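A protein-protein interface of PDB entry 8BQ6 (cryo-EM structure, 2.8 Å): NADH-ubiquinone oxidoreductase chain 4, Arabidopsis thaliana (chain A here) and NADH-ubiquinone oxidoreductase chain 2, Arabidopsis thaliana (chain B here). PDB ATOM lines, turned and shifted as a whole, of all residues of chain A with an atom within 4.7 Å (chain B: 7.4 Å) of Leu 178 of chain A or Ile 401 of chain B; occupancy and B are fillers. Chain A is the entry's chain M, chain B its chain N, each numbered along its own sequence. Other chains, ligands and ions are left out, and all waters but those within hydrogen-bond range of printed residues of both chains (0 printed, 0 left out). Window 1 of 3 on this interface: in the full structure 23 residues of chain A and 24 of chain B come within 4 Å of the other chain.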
ATOM      1  N   GLU A 147     -19.621  26.214  13.713  1.00  0.00           N
ATOM      2  CA  GLU A 147     -18.688  25.774  14.749  1.00  0.00           C
ATOM      3  C   GLU A 147     -19.060  26.311  16.113  1.00  0.00           C
ATOM      4  O   GLU A 147     -18.704  25.701  17.126  1.00  0.00           O
ATOM      5  CB  GLU A 147     -17.259  26.191  14.445  1.00  0.00           C
ATOM      6  CG  GLU A 147     -16.645  25.401  13.371  1.00  0.00           C
ATOM      7  CD  GLU A 147     -16.881  26.070  12.079  1.00  0.00           C
ATOM      8  OE1 GLU A 147     -16.524  27.263  11.995  1.00  0.00           O
ATOM      9  OE2 GLU A 147     -17.458  25.441  11.172  1.00  0.00           O
ATOM     10  N   LEU A 150     -20.610  23.969  18.602  1.00  0.00           N
ATOM     11  CA  LEU A 150     -19.806  22.916  19.206  1.00  0.00           C
ATOM     12  C   LEU A 150     -19.574  23.174  20.684  1.00  0.00           C
ATOM     13  O   LEU A 150     -19.584  22.242  21.490  1.00  0.00           O
ATOM     14  CB  LEU A 150     -18.467  22.796  18.485  1.00  0.00           C
ATOM     15  CG  LEU A 150     -18.342  21.650  17.493  1.00  0.00           C
ATOM     16  CD1 LEU A 150     -19.584  21.587  16.628  1.00  0.00           C
ATOM     17  CD2 LEU A 150     -17.107  21.867  16.661  1.00  0.00           C
ATOM     18  N   ILE A 151     -19.350  24.428  21.057  1.00  0.00           N
ATOM     19  CA  ILE A 151     -19.071  24.785  22.445  1.00  0.00           C
ATOM     20  C   ILE A 151     -20.252  24.417  23.344  1.00  0.00           C
ATOM     21  O   ILE A 151     -20.072  23.627  24.289  1.00  0.00           O
ATOM     22  CB  ILE A 151     -18.701  26.274  22.554  1.00  0.00           C
ATOM     23  CG1 ILE A 151     -17.458  26.562  21.710  1.00  0.00           C
ATOM     24  CG2 ILE A 151     -18.532  26.676  24.004  1.00  0.00           C
ATOM     25  CD1 ILE A 151     -17.142  28.023  21.570  1.00  0.00           C
ATOM     26  N   PHE A 174     -16.513  16.587  19.439  1.00  0.00           N
ATOM     27  CA  PHE A 174     -15.806  17.838  19.185  1.00  0.00           C
ATOM     28  C   PHE A 174     -14.753  17.662  18.097  1.00  0.00           C
ATOM     29  O   PHE A 174     -14.690  18.450  17.147  1.00  0.00           O
ATOM     30  CB  PHE A 174     -15.172  18.349  20.482  1.00  0.00           C
ATOM     31  CG  PHE A 174     -15.044  19.847  20.554  1.00  0.00           C
ATOM     32  CD1 PHE A 174     -14.325  20.544  19.602  1.00  0.00           C
ATOM     33  CD2 PHE A 174     -15.656  20.559  21.567  1.00  0.00           C
ATOM     34  CE1 PHE A 174     -14.209  21.916  19.667  1.00  0.00           C
ATOM     35  CE2 PHE A 174     -15.543  21.932  21.629  1.00  0.00           C
ATOM     36  CZ  PHE A 174     -14.816  22.608  20.678  1.00  0.00           C
ATOM     37  N   LEU A 175     -13.946  16.604  18.197  1.00  0.00           N
ATOM     38  CA  LEU A 175     -12.790  16.469  17.315  1.00  0.00           C
ATOM     39  C   LEU A 175     -13.202  16.141  15.881  1.00  0.00           C
ATOM     40  O   LEU A 175     -12.676  16.735  14.929  1.00  0.00           O
ATOM     41  CB  LEU A 175     -11.844  15.411  17.876  1.00  0.00           C
ATOM     42  CG  LEU A 175     -11.117  15.915  19.126  1.00  0.00           C
ATOM     43  CD1 LEU A 175     -10.552  14.773  19.949  1.00  0.00           C
ATOM     44  CD2 LEU A 175     -10.027  16.884  18.739  1.00  0.00           C
ATOM     45  N   TYR A 176     -14.145  15.207  15.705  1.00  0.00           N
ATOM     46  CA  TYR A 176     -14.650  14.904  14.367  1.00  0.00           C
ATOM     47  C   TYR A 176     -15.264  16.136  13.714  1.00  0.00           C
ATOM     48  O   TYR A 176     -14.955  16.468  12.555  1.00  0.00           O
ATOM     49  CB  TYR A 176     -15.696  13.796  14.439  1.00  0.00           C
ATOM     50  CG  TYR A 176     -15.199  12.402  14.179  1.00  0.00           C
ATOM     51  CD1 TYR A 176     -15.093  11.916  12.886  1.00  0.00           C
ATOM     52  CD2 TYR A 176     -14.893  11.552  15.226  1.00  0.00           C
ATOM     53  CE1 TYR A 176     -14.662  10.634  12.646  1.00  0.00           C
ATOM     54  CE2 TYR A 176     -14.465  10.270  14.996  1.00  0.00           C
ATOM     55  CZ  TYR A 176     -14.350   9.815  13.706  1.00  0.00           C
ATOM     56  OH  TYR A 176     -13.921   8.532  13.481  1.00  0.00           O
ATOM     57  N   THR A 177     -16.165  16.816  14.433  1.00  0.00           N
ATOM     58  CA  THR A 177     -16.833  17.961  13.831  1.00  0.00           C
ATOM     59  C   THR A 177     -15.841  19.065  13.497  1.00  0.00           C
ATOM     60  O   THR A 177     -15.960  19.721  12.454  1.00  0.00           O
ATOM     61  CB  THR A 177     -17.929  18.484  14.752  1.00  0.00           C
ATOM     62  OG1 THR A 177     -18.695  17.383  15.255  1.00  0.00           O
ATOM     63  CG2 THR A 177     -18.840  19.410  13.982  1.00  0.00           C
ATOM     64  N   LEU A 178     -14.853  19.286  14.369  1.00  0.00           N
ATOM     65  CA  LEU A 178     -13.874  20.331  14.107  1.00  0.00           C
ATOM     66  C   LEU A 178     -13.040  20.012  12.874  1.00  0.00           C
ATOM     67  O   LEU A 178     -12.806  20.892  12.037  1.00  0.00           O
ATOM     68  CB  LEU A 178     -12.982  20.531  15.328  1.00  0.00           C
ATOM     69  CG  LEU A 178     -11.830  21.504  15.108  1.00  0.00           C
ATOM     70  CD1 LEU A 178     -12.294  22.932  15.304  1.00  0.00           C
ATOM     71  CD2 LEU A 178     -10.700  21.171  16.040  1.00  0.00           C
ATOM     72  N   LEU A 179     -12.589  18.761  12.743  1.00  0.00           N
ATOM     73  CA  LEU A 179     -11.871  18.347  11.538  1.00  0.00           C
ATOM     74  C   LEU A 179     -12.673  18.664  10.280  1.00  0.00           C
ATOM     75  O   LEU A 179     -12.162  19.278   9.323  1.00  0.00           O
ATOM     76  CB  LEU A 179     -11.576  16.853  11.616  1.00  0.00           C
ATOM     77  CG  LEU A 179     -10.539  16.260  10.668  1.00  0.00           C
ATOM     78  CD1 LEU A 179      -9.208  16.971  10.819  1.00  0.00           C
ATOM     79  CD2 LEU A 179     -10.401  14.785  10.964  1.00  0.00           C
ATOM     80  N   GLY A 180     -13.942  18.246  10.262  1.00  0.00           N
ATOM     81  CA  GLY A 180     -14.761  18.508   9.090  1.00  0.00           C
ATOM     82  C   GLY A 180     -14.882  19.990   8.783  1.00  0.00           C
ATOM     83  O   GLY A 180     -14.670  20.425   7.640  1.00  0.00           O
ATOM     84  N   SER A 181     -15.189  20.792   9.804  1.00  0.00           N
ATOM     85  CA  SER A 181     -15.338  22.225   9.582  1.00  0.00           C
ATOM     86  C   SER A 181     -14.039  22.854   9.086  1.00  0.00           C
ATOM     87  O   SER A 181     -14.069  23.820   8.315  1.00  0.00           O
ATOM     88  CB  SER A 181     -15.822  22.906  10.858  1.00  0.00           C
ATOM     89  OG  SER A 181     -15.327  22.254  12.009  1.00  0.00           O
ATOM     90  N   LEU A 182     -12.900  22.239   9.406  1.00  0.00           N
ATOM     91  CA  LEU A 182     -11.588  22.799   8.978  1.00  0.00           C
ATOM     92  C   LEU A 182     -11.406  22.622   7.466  1.00  0.00           C
ATOM     93  O   LEU A 182     -10.861  23.543   6.841  1.00  0.00           O
ATOM     94  CB  LEU A 182     -10.461  22.125   9.767  1.00  0.00           C
ATOM     95  CG  LEU A 182     -10.175  22.744  11.134  1.00  0.00           C
ATOM     96  CD1 LEU A 182      -8.974  22.092  11.793  1.00  0.00           C
ATOM     97  CD2 LEU A 182      -9.977  24.246  11.023  1.00  0.00           C
ATOM     98  N   ILE B 393     -13.871  30.142  28.077  1.00  0.00           N
ATOM     99  CA  ILE B 393     -13.853  31.107  26.941  1.00  0.00           C
ATOM    100  C   ILE B 393     -12.405  31.289  26.465  1.00  0.00           C
ATOM    101  O   ILE B 393     -12.184  31.184  25.256  1.00  0.00           O
ATOM    102  CB  ILE B 393     -14.511  32.436  27.369  1.00  0.00           C
ATOM    103  CG1 ILE B 393     -16.033  32.319  27.467  1.00  0.00           C
ATOM    104  CG2 ILE B 393     -14.109  33.584  26.459  1.00  0.00           C
ATOM    105  CD1 ILE B 393     -16.675  33.455  28.227  1.00  0.00           C
ATOM    106  N   MET B 395      -9.808  29.241  26.794  1.00  0.00           N
ATOM    107  CA  MET B 395      -9.334  27.975  26.176  1.00  0.00           C
ATOM    108  C   MET B 395      -9.966  27.786  24.796  1.00  0.00           C
ATOM    109  O   MET B 395      -9.249  27.329  23.897  1.00  0.00           O
ATOM    110  CB  MET B 395      -9.692  26.766  27.044  1.00  0.00           C
ATOM    111  CG  MET B 395      -8.948  26.720  28.357  1.00  0.00           C
ATOM    112  SD  MET B 395      -7.217  26.293  28.110  1.00  0.00           S
ATOM    113  CE  MET B 395      -6.431  27.856  28.497  1.00  0.00           C
ATOM    114  N   PHE B 396     -11.253  28.099  24.638  1.00  0.00           N
ATOM    115  CA  PHE B 396     -11.828  27.987  23.304  1.00  0.00           C
ATOM    116  C   PHE B 396     -11.262  29.047  22.375  1.00  0.00           C
ATOM    117  O   PHE B 396     -11.132  28.807  21.170  1.00  0.00           O
ATOM    118  CB  PHE B 396     -13.351  28.092  23.355  1.00  0.00           C
ATOM    119  CG  PHE B 396     -14.019  26.896  23.956  1.00  0.00           C
ATOM    120  CD1 PHE B 396     -13.798  25.633  23.444  1.00  0.00           C
ATOM    121  CD2 PHE B 396     -14.883  27.036  25.024  1.00  0.00           C
ATOM    122  CE1 PHE B 396     -14.413  24.532  23.998  1.00  0.00           C
ATOM    123  CE2 PHE B 396     -15.497  25.940  25.581  1.00  0.00           C
ATOM    124  CZ  PHE B 396     -15.265  24.688  25.067  1.00  0.00           C
ATOM    125  N   SER B 397     -10.925  30.220  22.913  1.00  0.00           N
ATOM    126  CA  SER B 397     -10.279  31.242  22.102  1.00  0.00           C
ATOM    127  C   SER B 397      -8.874  30.815  21.693  1.00  0.00           C
ATOM    128  O   SER B 397      -8.473  31.001  20.538  1.00  0.00           O
ATOM    129  CB  SER B 397     -10.251  32.559  22.871  1.00  0.00           C
ATOM    130  OG  SER B 397     -10.181  33.660  21.986  1.00  0.00           O
ATOM    131  N   TYR B 398      -8.112  30.240  22.630  1.00  0.00           N
ATOM    132  CA  TYR B 398      -6.806  29.672  22.300  1.00  0.00           C
ATOM    133  C   TYR B 398      -6.926  28.613  21.213  1.00  0.00           C
ATOM    134  O   TYR B 398      -6.044  28.486  20.355  1.00  0.00           O
ATOM    135  CB  TYR B 398      -6.169  29.043  23.538  1.00  0.00           C
ATOM    136  CG  TYR B 398      -5.239  29.928  24.334  1.00  0.00           C
ATOM    137  CD1 TYR B 398      -4.117  30.490  23.756  1.00  0.00           C
ATOM    138  CD2 TYR B 398      -5.464  30.161  25.678  1.00  0.00           C
ATOM    139  CE1 TYR B 398      -3.262  31.283  24.489  1.00  0.00           C
ATOM    140  CE2 TYR B 398      -4.613  30.950  26.423  1.00  0.00           C
ATOM    141  CZ  TYR B 398      -3.514  31.508  25.821  1.00  0.00           C
ATOM    142  OH  TYR B 398      -2.659  32.294  26.551  1.00  0.00           O
ATOM    143  N   ALA B 399      -7.996  27.819  21.257  1.00  0.00           N
ATOM    144  CA  ALA B 399      -8.176  26.765  20.270  1.00  0.00           C
ATOM    145  C   ALA B 399      -8.644  27.309  18.927  1.00  0.00           C
ATOM    146  O   ALA B 399      -8.608  26.577  17.931  1.00  0.00           O
ATOM    147  CB  ALA B 399      -9.161  25.722  20.795  1.00  0.00           C
ATOM    148  N   GLY B 400      -9.075  28.567  18.875  1.00  0.00           N
ATOM    149  CA  GLY B 400      -9.458  29.182  17.622  1.00  0.00           C
ATOM    150  C   GLY B 400     -10.887  28.959  17.189  1.00  0.00           C
ATOM    151  O   GLY B 400     -11.192  29.115  16.004  1.00  0.00           O
ATOM    152  N   ILE B 401     -11.779  28.609  18.110  1.00  0.00           N
ATOM    153  CA  ILE B 401     -13.181  28.347  17.793  1.00  0.00           C
ATOM    154  C   ILE B 401     -13.896  29.662  17.515  1.00  0.00           C
ATOM    155  O   ILE B 401     -13.952  30.530  18.396  1.00  0.00           O
ATOM    156  CB  ILE B 401     -13.864  27.582  18.936  1.00  0.00           C
ATOM    157  CG1 ILE B 401     -13.091  26.306  19.249  1.00  0.00           C
ATOM    158  CG2 ILE B 401     -15.291  27.246  18.577  1.00  0.00           C
ATOM    159  CD1 ILE B 401     -12.961  25.392  18.061  1.00  0.00           C
ATOM    160  N   PRO B 402     -14.461  29.857  16.327  1.00  0.00           N
ATOM    161  CA  PRO B 402     -15.205  31.086  16.052  1.00  0.00           C
ATOM    162  C   PRO B 402     -16.459  31.152  16.904  1.00  0.00           C
ATOM    163  O   PRO B 402     -16.958  30.121  17.377  1.00  0.00           O
ATOM    164  CB  PRO B 402     -15.550  30.967  14.559  1.00  0.00           C
ATOM    165  CG  PRO B 402     -15.455  29.514  14.270  1.00  0.00           C
ATOM    166  CD  PRO B 402     -14.340  29.015  15.127  1.00  0.00           C
ATOM    167  N   PRO B 403     -16.988  32.348  17.149  1.00  0.00           N
ATOM    168  CA  PRO B 403     -16.522  33.661  16.692  1.00  0.00           C
ATOM    169  C   PRO B 403     -15.586  34.321  17.697  1.00  0.00           C
ATOM    170  O   PRO B 403     -15.529  35.544  17.777  1.00  0.00           O
ATOM    171  CB  PRO B 403     -17.829  34.444  16.539  1.00  0.00           C
ATOM    172  CG  PRO B 403     -18.802  33.790  17.507  1.00  0.00           C
ATOM    173  CD  PRO B 403     -18.247  32.448  17.901  1.00  0.00           C
ATOM    174  N   LEU B 404     -14.850  33.547  18.488  1.00  0.00           N
ATOM    175  CA  LEU B 404     -13.921  34.141  19.435  1.00  0.00           C
ATOM    176  C   LEU B 404     -12.728  34.748  18.701  1.00  0.00           C
ATOM    177  O   LEU B 404     -12.457  34.446  17.535  1.00  0.00           O
ATOM    178  CB  LEU B 404     -13.461  33.104  20.459  1.00  0.00           C
ATOM    179  CG  LEU B 404     -14.610  32.499  21.268  1.00  0.00           C
ATOM    180  CD1 LEU B 404     -14.113  31.456  22.244  1.00  0.00           C
ATOM    181  CD2 LEU B 404     -15.384  33.585  21.991  1.00  0.00           C
ATOM    182  N   ALA B 405     -12.031  35.664  19.378  1.00  0.00           N
ATOM    183  CA  ALA B 405     -10.919  36.416  18.746  1.00  0.00           C
ATOM    184  C   ALA B 405      -9.827  35.482  18.213  1.00  0.00           C
ATOM    185  O   ALA B 405      -9.186  35.858  17.226  1.00  0.00           O
ATOM    186  CB  ALA B 405     -10.368  37.416  19.740  1.00  0.00           C
ATOM    187  N   GLY B 406      -9.637  34.312  18.828  1.00  0.00           N
ATOM    188  CA  GLY B 406      -8.590  33.366  18.400  1.00  0.00           C
ATOM    189  C   GLY B 406      -8.783  32.863  16.981  1.00  0.00           C
ATOM    190  O   GLY B 406      -7.771  32.522  16.347  1.00  0.00           O
ATOM    191  N   PHE B 407     -10.031  32.798  16.502  1.00  0.00           N
ATOM    192  CA  PHE B 407     -10.300  32.398  15.099  1.00  0.00           C
ATOM    193  C   PHE B 407      -9.534  33.308  14.136  1.00  0.00           C
ATOM    194  O   PHE B 407      -8.908  32.770  13.233  1.00  0.00           O
ATOM    195  CB  PHE B 407     -11.801  32.417  14.811  1.00  0.00           C
ATOM    196  CG  PHE B 407     -12.143  32.231  13.357  1.00  0.00           C
ATOM    197  CD1 PHE B 407     -11.804  31.060  12.701  1.00  0.00           C
ATOM    198  CD2 PHE B 407     -12.769  33.237  12.640  1.00  0.00           C
ATOM    199  CE1 PHE B 407     -12.089  30.899  11.356  1.00  0.00           C
ATOM    200  CE2 PHE B 407     -13.059  33.070  11.297  1.00  0.00           C
ATOM    201  CZ  PHE B 407     -12.725  31.899  10.661  1.00  0.00           C
ATOM    202  N   CYS B 408      -9.616  34.626  14.303  1.00  0.00           N
ATOM    203  CA  CYS B 408      -8.922  35.601  13.413  1.00  0.00           C
ATOM    204  C   CYS B 408      -7.536  35.101  12.993  1.00  0.00           C
ATOM    205  O   CYS B 408      -7.297  35.006  11.779  1.00  0.00           O
ATOM    206  CB  CYS B 408      -8.763  36.944  14.113  1.00  0.00           C
ATOM    207  SG  CYS B 408     -10.336  37.766  14.463  1.00  0.00           S
ATOM    208  N   LYS B 410      -6.095  32.046  13.336  1.00  0.00           N
ATOM    209  CA  LYS B 410      -6.226  30.738  12.640  1.00  0.00           C
ATOM    210  C   LYS B 410      -6.680  30.969  11.194  1.00  0.00           C
ATOM    211  O   LYS B 410      -6.087  30.361  10.298  1.00  0.00           O
ATOM    212  CB  LYS B 410      -7.219  29.852  13.401  1.00  0.00           C
ATOM    213  CG  LYS B 410      -7.430  28.450  12.846  1.00  0.00           C
ATOM    214  CD  LYS B 410      -8.596  27.729  13.491  1.00  0.00           C
ATOM    215  CE  LYS B 410      -9.870  27.832  12.682  1.00  0.00           C
ATOM    216  NZ  LYS B 410     -11.053  27.348  13.434  1.00  0.00           N
ATOM    217  N   VAL B 430      -4.045  22.112   9.862  1.00  0.00           N
ATOM    218  CA  VAL B 430      -5.285  21.354  10.198  1.00  0.00           C
ATOM    219  C   VAL B 430      -4.977  20.348  11.312  1.00  0.00           C
ATOM    220  O   VAL B 430      -5.747  20.310  12.273  1.00  0.00           O
ATOM    221  CB  VAL B 430      -5.884  20.688   8.942  1.00  0.00           C
ATOM    222  CG1 VAL B 430      -6.815  19.530   9.264  1.00  0.00           C
ATOM    223  CG2 VAL B 430      -6.588  21.698   8.050  1.00  0.00           C
ATOM    224  N   SER B 433      -4.007  22.185  14.645  1.00  0.00           N
ATOM    225  CA  SER B 433      -5.187  22.826  15.204  1.00  0.00           C
ATOM    226  C   SER B 433      -6.072  21.811  15.911  1.00  0.00           C
ATOM    227  O   SER B 433      -6.600  22.087  16.993  1.00  0.00           O
ATOM    228  CB  SER B 433      -5.974  23.533  14.104  1.00  0.00           C
ATOM    229  OG  SER B 433      -5.404  24.788  13.787  1.00  0.00           O
ATOM    230  N   VAL B 434      -6.254  20.633  15.312  1.00  0.00           N
ATOM    231  CA  VAL B 434      -7.060  19.613  15.978  1.00  0.00           C
ATOM    232  C   VAL B 434      -6.408  19.183  17.294  1.00  0.00           C
ATOM    233  O   VAL B 434      -7.082  19.051  18.328  1.00  0.00           O
ATOM    234  CB  VAL B 434      -7.291  18.422  15.031  1.00  0.00           C
ATOM    235  CG1 VAL B 434      -7.909  17.260  15.780  1.00  0.00           C
ATOM    236  CG2 VAL B 434      -8.172  18.838  13.864  1.00  0.00           C
ATOM    237  N   ILE B 435      -5.091  18.966  17.281  1.00  0.00           N
ATOM    238  CA  ILE B 435      -4.395  18.564  18.505  1.00  0.00           C
ATOM    239  C   ILE B 435      -4.525  19.640  19.581  1.00  0.00           C
ATOM    240  O   ILE B 435      -4.776  19.344  20.763  1.00  0.00           O
ATOM    241  CB  ILE B 435      -2.920  18.254  18.200  1.00  0.00           C
ATOM    242  CG1 ILE B 435      -2.814  17.027  17.300  1.00  0.00           C
ATOM    243  CG2 ILE B 435      -2.147  18.042  19.488  1.00  0.00           C
ATOM    244  CD1 ILE B 435      -1.495  16.919  16.591  1.00  0.00           C
ATOM    245  N   GLY B 436      -4.336  20.902  19.191  1.00  0.00           N
ATOM    246  CA  GLY B 436      -4.489  21.990  20.136  1.00  0.00           C
ATOM    247  C   GLY B 436      -5.884  22.053  20.715  1.00  0.00           C
ATOM    248  O   GLY B 436      -6.055  22.223  21.924  1.00  0.00           O
ATOM    249  N   CYS B 437      -6.898  21.912  19.862  1.00  0.00           N
ATOM    250  CA  CYS B 437      -8.271  21.878  20.342  1.00  0.00           C
ATOM    251  C   CYS B 437      -8.450  20.794  21.393  1.00  0.00           C
ATOM    252  O   CYS B 437      -9.102  21.019  22.420  1.00  0.00           O
ATOM    253  CB  CYS B 437      -9.223  21.654  19.172  1.00  0.00           C
ATOM    254  SG  CYS B 437      -9.253  22.993  17.975  1.00  0.00           S
ATOM    255  N   PHE B 438      -7.858  19.620  21.167  1.00  0.00           N
ATOM    256  CA  PHE B 438      -7.989  18.544  22.145  1.00  0.00           C
ATOM    257  C   PHE B 438      -7.389  18.940  23.489  1.00  0.00           C
ATOM    258  O   PHE B 438      -8.042  18.824  24.538  1.00  0.00           O
ATOM    259  CB  PHE B 438      -7.321  17.270  21.639  1.00  0.00           C
ATOM    260  CG  PHE B 438      -7.143  16.231  22.705  1.00  0.00           C
ATOM    261  CD1 PHE B 438      -8.244  15.579  23.229  1.00  0.00           C
ATOM    262  CD2 PHE B 438      -5.889  15.915  23.195  1.00  0.00           C
ATOM    263  CE1 PHE B 438      -8.103  14.628  24.208  1.00  0.00           C
ATOM    264  CE2 PHE B 438      -5.741  14.959  24.183  1.00  0.00           C
ATOM    265  CZ  PHE B 438      -6.853  14.316  24.688  1.00  0.00           C
ATOM    266  N   ILE B 441      -9.558  21.722  25.224  1.00  0.00           N
ATOM    267  CA  ILE B 441     -10.843  21.276  25.759  1.00  0.00           C
ATOM    268  C   ILE B 441     -10.684  20.247  26.867  1.00  0.00           C
ATOM    269  O   ILE B 441     -11.648  19.987  27.597  1.00  0.00           O
ATOM    270  CB  ILE B 441     -11.769  20.712  24.661  1.00  0.00           C
ATOM    271  CG1 ILE B 441     -11.223  19.404  24.090  1.00  0.00           C
ATOM    272  CG2 ILE B 441     -11.996  21.741  23.563  1.00  0.00           C
ATOM    273  CD1 ILE B 441     -12.195  18.691  23.181  1.00  0.00           C
ATOM    274  N   ILE B 476     -12.468  39.189  24.081  1.00  0.00           N
ATOM    275  CA  ILE B 476     -12.318  37.890  23.430  1.00  0.00           C
ATOM    276  C   ILE B 476     -13.639  37.433  22.822  1.00  0.00           C
ATOM    277  O   ILE B 476     -13.667  36.860  21.725  1.00  0.00           O
ATOM    278  CB  ILE B 476     -11.754  36.856  24.422  1.00  0.00           C
ATOM    279  CG1 ILE B 476     -10.230  36.958  24.491  1.00  0.00           C
ATOM    280  CG2 ILE B 476     -12.171  35.443  24.049  1.00  0.00           C
ATOM    281  CD1 ILE B 476      -9.644  36.510  25.815  1.00  0.00           C
ATOM    282  N   LEU B 480     -14.826  40.186  17.190  1.00  0.00           N
ATOM    283  CA  LEU B 480     -15.212  39.948  15.771  1.00  0.00           C
ATOM    284  C   LEU B 480     -16.462  40.754  15.402  1.00  0.00           C
ATOM    285  O   LEU B 480     -16.785  40.776  14.209  1.00  0.00           O
ATOM    286  CB  LEU B 480     -15.414  38.445  15.544  1.00  0.00           C
ATOM    287  CG  LEU B 480     -14.128  37.662  15.277  1.00  0.00           C
ATOM    288  CD1 LEU B 480     -14.427  36.335  14.601  1.00  0.00           C
ATOM    289  CD2 LEU B 480     -13.162  38.476  14.431  1.00  0.00           C
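Printed residues of chain B within 4 Å of Phe 174 of chain A: Phe 396.
Thr 177 of chain A touches none of the printed residues of chain B.
Printed residues of chain A within 4 Å of Ile 401 of chain B: Ile 151 and Leu 178.
Of the printed residues of chain A, Pro 402 of chain B touches Glu 147.
Printed residues of chain A within 4 Å of Lys 410 of chain B: Leu 182.
Printed residues of chain A within 4 Å of Val 430 of chain B: Leu 179 (3.8 Å) and Leu 182 (3.7 Å).
Of the printed residues of chain A, Val 434 of chain B touches Leu 175, Leu 178, Leu 179 and Leu 182.
Gly 436 of chain B touches none of the printed residues of chain A.
The nearest residue of chain B that does not touch Leu 178 of chain A is Ser 433 of chain B (4.3 Å).
The nearest printed residue of chain A that does not touch Ile 401 of chain B is Glu 147 of chain A (4.02 Å).
Of the 26 printed residues of chain B, 8 touch a printed residue of chain A.
Hydrophobic or aromatic side chains of chain B within 4 Å of the printed part of chain A: Phe 396, Ile 401, Pro 402, Val 430, Val 434 and Phe 438.
Among the printed residues, no Asp or Glu carboxylate lies within 4 Å of a Lys or Arg side-chain nitrogen of the other chain.
Among the printed residues, merely in contact across the chains: Leu 178 of chain A with Cys 437 of chain B (3.0 Å), Glu 147 of chain A with Pro 402 of chain B (3.4 Å), Ile 151 of chain A with Phe 396 of chain B (3.5 Å), Ile 151 of chain A with Ile 401 of chain B (3.6 Å), Leu 175 of chain A with Val 434 of chain B (3.7 Å), Phe 174 of chain A with Phe 396 of chain B (3.7 Å), Leu 182 of chain A with Val 430 of chain B (3.7 Å), Leu 179 of chain A with Val 434 of chain B (3.7 Å), Leu 178 of chain A with Ile 401 of chain B (3.8 Å), Leu 179 of chain A with Val 430 of chain B (3.8 Å), Leu 182 of chain A with Val 434 of chain B (3.9 Å), Leu 182 of chain A with Lys 410 of chain B (3.95 Å), Leu 178 of chain A with Val 434 of chain B (3.96 Å) and Leu 175 of chain A with Phe 438 of chain B (3.99 Å).
The backbone carbonyl oxygen (O) of Leu 178 of chain A lies within hydrogen-bond range of the side-chain hydroxyl (OG) of Ser 181 of chain A.
The backbone carbonyl oxygen (O) of Gly 400 of chain B lies within hydrogen-bond range of the side-chain amino group (NZ) of Lys 410 of chain B, 3.1 Å away.
N of Ile 401 of chain B sits at hydrogen-bond distance from O of Phe 396 of chain B (3.1 Å).
SG of Cys 437 of chain B lies within hydrogen-bond range of O of Ala 399 of chain B (3.6 Å).
The backbone carbonyl oxygen (O) of Ser 433 of chain B sits at hydrogen-bond distance from the side-chain sulfur (SG) of Cys 437 of chain B, at 3.0 Å.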
